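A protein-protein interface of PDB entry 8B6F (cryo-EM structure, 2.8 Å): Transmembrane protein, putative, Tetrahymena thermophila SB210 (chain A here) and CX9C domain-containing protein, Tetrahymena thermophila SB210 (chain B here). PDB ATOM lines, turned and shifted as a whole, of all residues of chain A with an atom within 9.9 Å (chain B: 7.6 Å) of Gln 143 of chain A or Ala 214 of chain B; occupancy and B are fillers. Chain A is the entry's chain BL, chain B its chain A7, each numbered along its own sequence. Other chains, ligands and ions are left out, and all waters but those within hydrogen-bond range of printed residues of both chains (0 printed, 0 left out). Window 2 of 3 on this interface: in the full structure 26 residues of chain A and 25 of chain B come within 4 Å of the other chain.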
ATOM      1  N   ASP A  19     -17.467  11.001   7.766  1.00  0.00           N
ATOM      2  CA  ASP A  19     -16.038  10.987   7.459  1.00  0.00           C
ATOM      3  C   ASP A  19     -15.827  11.709   6.136  1.00  0.00           C
ATOM      4  O   ASP A  19     -15.657  11.072   5.087  1.00  0.00           O
ATOM      5  CB  ASP A  19     -15.498   9.558   7.413  1.00  0.00           C
ATOM      6  CG  ASP A  19     -13.985   9.501   7.530  1.00  0.00           C
ATOM      7  OD1 ASP A  19     -13.346  10.575   7.538  1.00  0.00           O
ATOM      8  OD2 ASP A  19     -13.434   8.385   7.621  1.00  0.00           O
ATOM      9  N   GLU A  21     -13.231  13.192   5.074  1.00  0.00           N
ATOM     10  CA  GLU A  21     -11.939  12.800   4.523  1.00  0.00           C
ATOM     11  C   GLU A  21     -12.059  11.501   3.738  1.00  0.00           C
ATOM     12  O   GLU A  21     -11.536  11.384   2.625  1.00  0.00           O
ATOM     13  CB  GLU A  21     -10.912  12.661   5.645  1.00  0.00           C
ATOM     14  CG  GLU A  21      -9.503  12.378   5.155  1.00  0.00           C
ATOM     15  CD  GLU A  21      -8.492  12.342   6.282  1.00  0.00           C
ATOM     16  OE1 GLU A  21      -8.895  12.533   7.448  1.00  0.00           O
ATOM     17  OE2 GLU A  21      -7.293  12.123   6.004  1.00  0.00           O
ATOM     18  N   ASN A  22     -12.760  10.514   4.298  1.00  0.00           N
ATOM     19  CA  ASN A  22     -12.957   9.257   3.583  1.00  0.00           C
ATOM     20  C   ASN A  22     -13.744   9.473   2.299  1.00  0.00           C
ATOM     21  O   ASN A  22     -13.417   8.894   1.257  1.00  0.00           O
ATOM     22  CB  ASN A  22     -13.674   8.254   4.485  1.00  0.00           C
ATOM     23  CG  ASN A  22     -14.033   6.974   3.761  1.00  0.00           C
ATOM     24  OD1 ASN A  22     -13.329   6.545   2.848  1.00  0.00           O
ATOM     25  ND2 ASN A  22     -15.141   6.363   4.159  1.00  0.00           N
ATOM     26  N   ARG A  25     -11.429  10.961  -0.276  1.00  0.00           N
ATOM     27  CA  ARG A  25     -10.481   9.978  -0.788  1.00  0.00           C
ATOM     28  C   ARG A  25     -11.151   9.038  -1.781  1.00  0.00           C
ATOM     29  O   ARG A  25     -10.577   8.719  -2.829  1.00  0.00           O
ATOM     30  CB  ARG A  25      -9.862   9.191   0.368  1.00  0.00           C
ATOM     31  CG  ARG A  25      -8.975  10.037   1.272  1.00  0.00           C
ATOM     32  CD  ARG A  25      -8.160   9.190   2.237  1.00  0.00           C
ATOM     33  NE  ARG A  25      -8.971   8.217   2.958  1.00  0.00           N
ATOM     34  CZ  ARG A  25      -8.508   7.415   3.909  1.00  0.00           C
ATOM     35  NH1 ARG A  25      -7.245   7.465   4.300  1.00  0.00           N
ATOM     36  NH2 ARG A  25      -9.333   6.542   4.479  1.00  0.00           N
ATOM     37  N   LEU A  28     -11.762  10.906  -5.031  1.00  0.00           N
ATOM     38  CA  LEU A  28     -10.503  11.062  -5.752  1.00  0.00           C
ATOM     39  C   LEU A  28     -10.078   9.754  -6.404  1.00  0.00           C
ATOM     40  O   LEU A  28      -9.592   9.749  -7.541  1.00  0.00           O
ATOM     41  CB  LEU A  28      -9.415  11.563  -4.802  1.00  0.00           C
ATOM     42  CG  LEU A  28      -8.003  11.648  -5.388  1.00  0.00           C
ATOM     43  CD1 LEU A  28      -7.967  12.561  -6.601  1.00  0.00           C
ATOM     44  CD2 LEU A  28      -7.024  12.128  -4.331  1.00  0.00           C
ATOM     45  N   ALA A  29     -10.254   8.634  -5.703  1.00  0.00           N
ATOM     46  CA  ALA A  29      -9.880   7.345  -6.275  1.00  0.00           C
ATOM     47  C   ALA A  29     -10.669   7.058  -7.544  1.00  0.00           C
ATOM     48  O   ALA A  29     -10.101   6.646  -8.561  1.00  0.00           O
ATOM     49  CB  ALA A  29     -10.100   6.238  -5.245  1.00  0.00           C
ATOM     50  N   ASN A  32      -9.563   9.318 -10.384  1.00  0.00           N
ATOM     51  CA  ASN A  32      -8.320   8.836 -10.977  1.00  0.00           C
ATOM     52  C   ASN A  32      -8.569   7.624 -11.864  1.00  0.00           C
ATOM     53  O   ASN A  32      -7.978   7.502 -12.943  1.00  0.00           O
ATOM     54  CB  ASN A  32      -7.313   8.493  -9.878  1.00  0.00           C
ATOM     55  CG  ASN A  32      -6.884   9.708  -9.085  1.00  0.00           C
ATOM     56  OD1 ASN A  32      -7.576  10.724  -9.061  1.00  0.00           O
ATOM     57  ND2 ASN A  32      -5.732   9.612  -8.432  1.00  0.00           N
ATOM     58  N   ASP A 124     -10.793  -4.244  -5.975  1.00  0.00           N
ATOM     59  CA  ASP A 124     -10.602  -3.300  -4.878  1.00  0.00           C
ATOM     60  C   ASP A 124     -11.545  -2.110  -5.001  1.00  0.00           C
ATOM     61  O   ASP A 124     -12.144  -1.678  -4.010  1.00  0.00           O
ATOM     62  CB  ASP A 124      -9.147  -2.835  -4.830  1.00  0.00           C
ATOM     63  CG  ASP A 124      -8.687  -2.215  -6.132  1.00  0.00           C
ATOM     64  OD1 ASP A 124      -9.520  -2.072  -7.050  1.00  0.00           O
ATOM     65  OD2 ASP A 124      -7.493  -1.867  -6.236  1.00  0.00           O
ATOM     66  N   ASP A 133     -15.987   2.466   3.143  1.00  0.00           N
ATOM     67  CA  ASP A 133     -14.578   2.723   3.396  1.00  0.00           C
ATOM     68  C   ASP A 133     -13.798   2.798   2.092  1.00  0.00           C
ATOM     69  O   ASP A 133     -14.040   2.025   1.162  1.00  0.00           O
ATOM     70  CB  ASP A 133     -13.982   1.631   4.286  1.00  0.00           C
ATOM     71  CG  ASP A 133     -14.609   1.598   5.664  1.00  0.00           C
ATOM     72  OD1 ASP A 133     -15.428   2.491   5.970  1.00  0.00           O
ATOM     73  OD2 ASP A 133     -14.285   0.677   6.444  1.00  0.00           O
ATOM     74  N   ALA A 134     -12.861   3.738   2.034  1.00  0.00           N
ATOM     75  CA  ALA A 134     -11.927   3.842   0.924  1.00  0.00           C
ATOM     76  C   ALA A 134     -10.647   3.057   1.166  1.00  0.00           C
ATOM     77  O   ALA A 134      -9.754   3.076   0.313  1.00  0.00           O
ATOM     78  CB  ALA A 134     -11.586   5.312   0.662  1.00  0.00           C
ATOM     79  N   ARG A 135     -10.538   2.370   2.306  1.00  0.00           N
ATOM     80  CA  ARG A 135      -9.339   1.603   2.616  1.00  0.00           C
ATOM     81  C   ARG A 135      -9.130   0.438   1.659  1.00  0.00           C
ATOM     82  O   ARG A 135      -8.016  -0.088   1.581  1.00  0.00           O
ATOM     83  CB  ARG A 135      -9.407   1.088   4.052  1.00  0.00           C
ATOM     84  CG  ARG A 135      -9.176   2.167   5.090  1.00  0.00           C
ATOM     85  CD  ARG A 135      -9.346   1.649   6.509  1.00  0.00           C
ATOM     86  NE  ARG A 135     -10.736   1.346   6.822  1.00  0.00           N
ATOM     87  CZ  ARG A 135     -11.180   1.020   8.028  1.00  0.00           C
ATOM     88  NH1 ARG A 135     -10.367   0.954   9.070  1.00  0.00           N
ATOM     89  NH2 ARG A 135     -12.472   0.757   8.195  1.00  0.00           N
ATOM     90  N   TYR A 136     -10.171   0.017   0.940  1.00  0.00           N
ATOM     91  CA  TYR A 136     -10.013  -1.068  -0.020  1.00  0.00           C
ATOM     92  C   TYR A 136      -9.214  -0.647  -1.245  1.00  0.00           C
ATOM     93  O   TYR A 136      -8.683  -1.514  -1.947  1.00  0.00           O
ATOM     94  CB  TYR A 136     -11.384  -1.579  -0.464  1.00  0.00           C
ATOM     95  CG  TYR A 136     -12.230  -2.128   0.659  1.00  0.00           C
ATOM     96  CD1 TYR A 136     -12.135  -3.459   1.038  1.00  0.00           C
ATOM     97  CD2 TYR A 136     -13.133  -1.317   1.331  1.00  0.00           C
ATOM     98  CE1 TYR A 136     -12.909  -3.965   2.060  1.00  0.00           C
ATOM     99  CE2 TYR A 136     -13.914  -1.816   2.356  1.00  0.00           C
ATOM    100  CZ  TYR A 136     -13.797  -3.142   2.715  1.00  0.00           C
ATOM    101  OH  TYR A 136     -14.571  -3.646   3.734  1.00  0.00           O
ATOM    102  N   CYS A 137      -9.102   0.652  -1.509  1.00  0.00           N
ATOM    103  CA  CYS A 137      -8.506   1.182  -2.732  1.00  0.00           C
ATOM    104  C   CYS A 137      -7.399   2.174  -2.396  1.00  0.00           C
ATOM    105  O   CYS A 137      -7.347   3.288  -2.918  1.00  0.00           O
ATOM    106  CB  CYS A 137      -9.568   1.831  -3.613  1.00  0.00           C
ATOM    107  SG  CYS A 137     -10.507   3.144  -2.809  1.00  0.00           S
ATOM    108  N   ILE A 138      -6.491   1.770  -1.505  1.00  0.00           N
ATOM    109  CA  ILE A 138      -5.438   2.673  -1.049  1.00  0.00           C
ATOM    110  C   ILE A 138      -4.624   3.194  -2.227  1.00  0.00           C
ATOM    111  O   ILE A 138      -4.276   4.380  -2.284  1.00  0.00           O
ATOM    112  CB  ILE A 138      -4.544   1.963  -0.014  1.00  0.00           C
ATOM    113  CG1 ILE A 138      -5.323   1.717   1.279  1.00  0.00           C
ATOM    114  CG2 ILE A 138      -3.284   2.776   0.270  1.00  0.00           C
ATOM    115  CD1 ILE A 138      -4.605   0.822   2.269  1.00  0.00           C
ATOM    116  N   SER A 139      -4.307   2.322  -3.185  1.00  0.00           N
ATOM    117  CA  SER A 139      -3.407   2.710  -4.265  1.00  0.00           C
ATOM    118  C   SER A 139      -3.967   3.856  -5.097  1.00  0.00           C
ATOM    119  O   SER A 139      -3.198   4.656  -5.642  1.00  0.00           O
ATOM    120  CB  SER A 139      -3.116   1.505  -5.160  1.00  0.00           C
ATOM    121  OG  SER A 139      -4.311   0.969  -5.703  1.00  0.00           O
ATOM    122  N   TRP A 140      -5.293   3.960  -5.208  1.00  0.00           N
ATOM    123  CA  TRP A 140      -5.882   4.884  -6.171  1.00  0.00           C
ATOM    124  C   TRP A 140      -5.828   6.338  -5.715  1.00  0.00           C
ATOM    125  O   TRP A 140      -5.727   7.234  -6.560  1.00  0.00           O
ATOM    126  CB  TRP A 140      -7.326   4.480  -6.466  1.00  0.00           C
ATOM    127  CG  TRP A 140      -7.419   3.234  -7.289  1.00  0.00           C
ATOM    128  CD1 TRP A 140      -7.671   1.972  -6.839  1.00  0.00           C
ATOM    129  CD2 TRP A 140      -7.251   3.128  -8.708  1.00  0.00           C
ATOM    130  NE1 TRP A 140      -7.672   1.086  -7.889  1.00  0.00           N
ATOM    131  CE2 TRP A 140      -7.417   1.771  -9.048  1.00  0.00           C
ATOM    132  CE3 TRP A 140      -6.977   4.050  -9.725  1.00  0.00           C
ATOM    133  CZ2 TRP A 140      -7.320   1.312 -10.359  1.00  0.00           C
ATOM    134  CZ3 TRP A 140      -6.882   3.594 -11.028  1.00  0.00           C
ATOM    135  CH2 TRP A 140      -7.052   2.236 -11.334  1.00  0.00           C
ATOM    136  N   TRP A 141      -5.890   6.603  -4.412  1.00  0.00           N
ATOM    137  CA  TRP A 141      -5.876   7.975  -3.901  1.00  0.00           C
ATOM    138  C   TRP A 141      -4.500   8.385  -3.385  1.00  0.00           C
ATOM    139  O   TRP A 141      -4.384   9.111  -2.395  1.00  0.00           O
ATOM    140  CB  TRP A 141      -6.944   8.174  -2.825  1.00  0.00           C
ATOM    141  CG  TRP A 141      -7.036   7.102  -1.786  1.00  0.00           C
ATOM    142  CD1 TRP A 141      -7.803   5.977  -1.840  1.00  0.00           C
ATOM    143  CD2 TRP A 141      -6.355   7.065  -0.526  1.00  0.00           C
ATOM    144  NE1 TRP A 141      -7.639   5.238  -0.695  1.00  0.00           N
ATOM    145  CE2 TRP A 141      -6.755   5.884   0.128  1.00  0.00           C
ATOM    146  CE3 TRP A 141      -5.444   7.914   0.109  1.00  0.00           C
ATOM    147  CZ2 TRP A 141      -6.274   5.528   1.385  1.00  0.00           C
ATOM    148  CZ3 TRP A 141      -4.968   7.561   1.358  1.00  0.00           C
ATOM    149  CH2 TRP A 141      -5.384   6.377   1.984  1.00  0.00           C
ATOM    150  N   LYS A 142      -3.441   7.930  -4.053  1.00  0.00           N
ATOM    151  CA  LYS A 142      -2.051   8.370  -3.918  1.00  0.00           C
ATOM    152  C   LYS A 142      -1.319   7.754  -2.728  1.00  0.00           C
ATOM    153  O   LYS A 142      -0.122   8.023  -2.575  1.00  0.00           O
ATOM    154  CB  LYS A 142      -1.926   9.901  -3.820  1.00  0.00           C
ATOM    155  CG  LYS A 142      -1.702  10.446  -2.407  1.00  0.00           C
ATOM    156  CD  LYS A 142      -1.872  11.957  -2.358  1.00  0.00           C
ATOM    157  CE  LYS A 142      -0.788  12.664  -3.159  1.00  0.00           C
ATOM    158  NZ  LYS A 142      -0.904  14.147  -3.058  1.00  0.00           N
ATOM    159  N   GLN A 143      -1.966   6.943  -1.900  1.00  0.00           N
ATOM    160  CA  GLN A 143      -1.255   6.269  -0.817  1.00  0.00           C
ATOM    161  C   GLN A 143      -1.020   4.811  -1.183  1.00  0.00           C
ATOM    162  O   GLN A 143      -0.192   4.128  -0.579  1.00  0.00           O
ATOM    163  CB  GLN A 143      -2.030   6.363   0.499  1.00  0.00           C
ATOM    164  CG  GLN A 143      -1.317   5.691   1.669  1.00  0.00           C
ATOM    165  CD  GLN A 143      -1.972   5.981   3.006  1.00  0.00           C
ATOM    166  OE1 GLN A 143      -2.722   6.945   3.148  1.00  0.00           O
ATOM    167  NE2 GLN A 143      -1.688   5.143   3.997  1.00  0.00           N
ATOM    168  OXT GLN A 143      -1.649   4.280  -2.096  1.00  0.00           O
ATOM    169  N   PHE B 208      -4.201  -6.649   5.382  1.00  0.00           N
ATOM    170  CA  PHE B 208      -5.028  -5.945   6.354  1.00  0.00           C
ATOM    171  C   PHE B 208      -4.208  -4.999   7.221  1.00  0.00           C
ATOM    172  O   PHE B 208      -4.763  -4.047   7.777  1.00  0.00           O
ATOM    173  CB  PHE B 208      -5.781  -6.943   7.231  1.00  0.00           C
ATOM    174  CG  PHE B 208      -6.991  -6.359   7.898  1.00  0.00           C
ATOM    175  CD1 PHE B 208      -8.139  -6.099   7.167  1.00  0.00           C
ATOM    176  CD2 PHE B 208      -6.981  -6.072   9.251  1.00  0.00           C
ATOM    177  CE1 PHE B 208      -9.254  -5.561   7.774  1.00  0.00           C
ATOM    178  CE2 PHE B 208      -8.092  -5.534   9.864  1.00  0.00           C
ATOM    179  CZ  PHE B 208      -9.231  -5.278   9.126  1.00  0.00           C
ATOM    180  N   ALA B 209      -2.904  -5.242   7.350  1.00  0.00           N
ATOM    181  CA  ALA B 209      -2.045  -4.304   8.062  1.00  0.00           C
ATOM    182  C   ALA B 209      -2.059  -2.940   7.383  1.00  0.00           C
ATOM    183  O   ALA B 209      -2.281  -1.912   8.032  1.00  0.00           O
ATOM    184  CB  ALA B 209      -0.621  -4.852   8.144  1.00  0.00           C
ATOM    185  N   GLU B 210      -1.831  -2.912   6.069  1.00  0.00           N
ATOM    186  CA  GLU B 210      -1.897  -1.650   5.338  1.00  0.00           C
ATOM    187  C   GLU B 210      -3.319  -1.106   5.316  1.00  0.00           C
ATOM    188  O   GLU B 210      -3.524   0.111   5.354  1.00  0.00           O
ATOM    189  CB  GLU B 210      -1.373  -1.840   3.914  1.00  0.00           C
ATOM    190  CG  GLU B 210       0.047  -2.380   3.846  1.00  0.00           C
ATOM    191  CD  GLU B 210       1.059  -1.448   4.485  1.00  0.00           C
ATOM    192  OE1 GLU B 210       0.716  -0.274   4.735  1.00  0.00           O
ATOM    193  OE2 GLU B 210       2.199  -1.889   4.738  1.00  0.00           O
ATOM    194  N   PHE B 211      -4.311  -1.994   5.243  1.00  0.00           N
ATOM    195  CA  PHE B 211      -5.704  -1.572   5.332  1.00  0.00           C
ATOM    196  C   PHE B 211      -5.936  -0.732   6.583  1.00  0.00           C
ATOM    197  O   PHE B 211      -6.515   0.358   6.520  1.00  0.00           O
ATOM    198  CB  PHE B 211      -6.612  -2.803   5.328  1.00  0.00           C
ATOM    199  CG  PHE B 211      -8.076  -2.486   5.256  1.00  0.00           C
ATOM    200  CD1 PHE B 211      -8.777  -2.112   6.389  1.00  0.00           C
ATOM    201  CD2 PHE B 211      -8.759  -2.593   4.057  1.00  0.00           C
ATOM    202  CE1 PHE B 211     -10.127  -1.831   6.324  1.00  0.00           C
ATOM    203  CE2 PHE B 211     -10.108  -2.314   3.984  1.00  0.00           C
ATOM    204  CZ  PHE B 211     -10.793  -1.932   5.121  1.00  0.00           C
ATOM    205  N   LEU B 212      -5.479  -1.228   7.734  1.00  0.00           N
ATOM    206  CA  LEU B 212      -5.649  -0.497   8.986  1.00  0.00           C
ATOM    207  C   LEU B 212      -4.759   0.738   9.035  1.00  0.00           C
ATOM    208  O   LEU B 212      -5.155   1.773   9.583  1.00  0.00           O
ATOM    209  CB  LEU B 212      -5.359  -1.413  10.175  1.00  0.00           C
ATOM    210  CG  LEU B 212      -6.306  -2.600  10.369  1.00  0.00           C
ATOM    211  CD1 LEU B 212      -5.882  -3.413  11.582  1.00  0.00           C
ATOM    212  CD2 LEU B 212      -7.754  -2.144  10.509  1.00  0.00           C
ATOM    213  N   GLU B 213      -3.552   0.651   8.472  1.00  0.00           N
ATOM    214  CA  GLU B 213      -2.654   1.801   8.484  1.00  0.00           C
ATOM    215  C   GLU B 213      -3.281   2.994   7.775  1.00  0.00           C
ATOM    216  O   GLU B 213      -3.165   4.133   8.242  1.00  0.00           O
ATOM    217  CB  GLU B 213      -1.324   1.431   7.827  1.00  0.00           C
ATOM    218  CG  GLU B 213      -0.439   0.531   8.676  1.00  0.00           C
ATOM    219  CD  GLU B 213       0.164   1.258   9.860  1.00  0.00           C
ATOM    220  OE1 GLU B 213      -0.110   2.465  10.021  1.00  0.00           O
ATOM    221  OE2 GLU B 213       0.913   0.621  10.631  1.00  0.00           O
ATOM    222  N   ALA B 214      -3.950   2.757   6.651  1.00  0.00           N
ATOM    223  CA  ALA B 214      -4.598   3.831   5.910  1.00  0.00           C
ATOM    224  C   ALA B 214      -5.966   4.152   6.496  1.00  0.00           C
ATOM    225  O   ALA B 214      -6.961   4.197   5.766  1.00  0.00           O
ATOM    226  CB  ALA B 214      -4.734   3.455   4.435  1.00  0.00           C
ATOM    227  N   SER B 215      -6.027   4.400   7.801  1.00  0.00           N
ATOM    228  CA  SER B 215      -7.282   4.639   8.502  1.00  0.00           C
ATOM    229  C   SER B 215      -7.355   6.091   8.946  1.00  0.00           C
ATOM    230  O   SER B 215      -6.344   6.689   9.325  1.00  0.00           O
ATOM    231  CB  SER B 215      -7.420   3.722   9.720  1.00  0.00           C
ATOM    232  OG  SER B 215      -7.488   2.361   9.334  1.00  0.00           O
ATOM    233  N   THR B 216      -8.557   6.653   8.894  1.00  0.00           N
ATOM    234  CA  THR B 216      -8.787   8.033   9.281  1.00  0.00           C
ATOM    235  C   THR B 216      -9.053   8.127  10.780  1.00  0.00           C
ATOM    236  O   THR B 216      -9.284   7.131  11.465  1.00  0.00           O
ATOM    237  CB  THR B 216      -9.958   8.624   8.498  1.00  0.00           C
ATOM    238  OG1 THR B 216     -11.155   7.894   8.794  1.00  0.00           O
ATOM    239  CG2 THR B 216      -9.687   8.562   7.005  1.00  0.00           C
ATOM    240  N   GLN B 219     -12.494   6.793  11.681  1.00  0.00           N
ATOM    241  CA  GLN B 219     -12.520   5.335  11.661  1.00  0.00           C
ATOM    242  C   GLN B 219     -11.800   4.746  12.867  1.00  0.00           C
ATOM    243  O   GLN B 219     -12.183   3.679  13.358  1.00  0.00           O
ATOM    244  CB  GLN B 219     -11.897   4.818  10.365  1.00  0.00           C
ATOM    245  CG  GLN B 219     -12.719   5.136   9.124  1.00  0.00           C
ATOM    246  CD  GLN B 219     -12.043   4.686   7.847  1.00  0.00           C
ATOM    247  OE1 GLN B 219     -10.825   4.523   7.799  1.00  0.00           O
ATOM    248  NE2 GLN B 219     -12.834   4.476   6.802  1.00  0.00           N
ATOM    249  N   LEU B 220     -10.758   5.419  13.356  1.00  0.00           N
ATOM    250  CA  LEU B 220     -10.035   4.980  14.549  1.00  0.00           C
ATOM    251  C   LEU B 220     -10.763   5.449  15.811  1.00  0.00           C
ATOM    252  O   LEU B 220     -10.238   6.200  16.632  1.00  0.00           O
ATOM    253  CB  LEU B 220      -8.605   5.499  14.515  1.00  0.00           C
ATOM    254  CG  LEU B 220      -7.748   5.045  13.334  1.00  0.00           C
ATOM    255  CD1 LEU B 220      -6.481   5.878  13.249  1.00  0.00           C
ATOM    256  CD2 LEU B 220      -7.412   3.568  13.445  1.00  0.00           C
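OD2 of Asp 19 of chain A touches CG of Gln 219 of chain B (3.7 Å).
Asn 22 of chain A touches Gln 219 of chain B (ND2 to NE2, 3.98 Å).
NH2 of Arg 25 of chain A touches O of Ala 214 of chain B (3.6 Å).
CG2 of Thr 216 of chain B touches NH2 of Arg 25 of chain A (3.3 Å).
CD of Arg 135 of chain A touches O of Phe 211 of chain B, 3.1 Å away.
Arg 135 of chain A touches Ala 214 of chain B.
Tyr 136 of chain A touches Phe 211 of chain B.
Ile 138 of chain A touches Ala 214 of chain B (CD1 to CB, 3.4 Å).
Ala 214 of chain B touches Trp 141 of chain A.
Ala 214 of chain B touches Gln 143 of chain A (CB to NE2, 3.5 Å).
OG1 of Thr 216 of chain B lies within hydrogen-bond range of OD2 of Asp 19 of chain A.
OD1 of Asp 133 of chain A sits at hydrogen-bond distance from NE2 of Gln 219 of chain B.
NH1 of Arg 135 of chain A is in hydrogen-bond range of OG of Ser 215 of chain B, at 3.2 Å.
The guanidinium group (NE) of Arg 135 of chain A sits at hydrogen-bond distance from the side-chain amide oxygen (OE1) of Gln 219 of chain B (3.3 Å).
The side-chain carboxylate (OD1) of Asp 19 of chain A is in hydrogen-bond range of the backbone NH (N) of Asn 22 of chain A (3.3 Å).
NH2 of Arg 135 of chain A is in salt-bridge range of OD2 of Asp 133 of chain A (2.5 Å).
The backbone carbonyl oxygen (O) of Ala 134 of chain A sits at hydrogen-bond distance from the indole nitrogen (NE1) of Trp 141 of chain A (3.2 Å).
The backbone carbonyl oxygen (O) of Cys 137 of chain A lies close to the indole nitrogen (NE1) of Trp 141 of chain A.
The backbone NH of Gln 143 of chain A lies close to the backbone carbonyl oxygen of Ile 138 of chain A.
O of Leu 212 of chain B lies within hydrogen-bond range of OG of Ser 215 of chain B, 2.4 Å away.
Of the printed residues of chain B, Arg 135 of chain A touches Phe 211 (3.1 Å), Ala 214 (3.1 Å), Ser 215 (3.2 Å) and Gln 219 (3.3 Å).
Of the printed residues of chain B, Gln 143 of chain A touches Ala 214 (3.5 Å).
Ser 215 of chain B touches just one residue of chain A: Arg 135.
Printed residues of chain A within 4 Å of Gln 219 of chain B: Asp 19 (3.7 Å), Asn 22 (3.98 Å), Asp 133 (3.4 Å) and Arg 135 (3.3 Å).
The nearest residue of chain B that does not touch Gln 143 of chain A is Glu 213 of chain B (4.6 Å).
Hydrophobic or aromatic side chains of chain A within 4 Å of the printed part of chain B: Tyr 136, Ile 138 and Trp 141.
Hydrophobic or aromatic side chains of chain B that line the printed part of chain A: Phe 211 and Ala 214.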
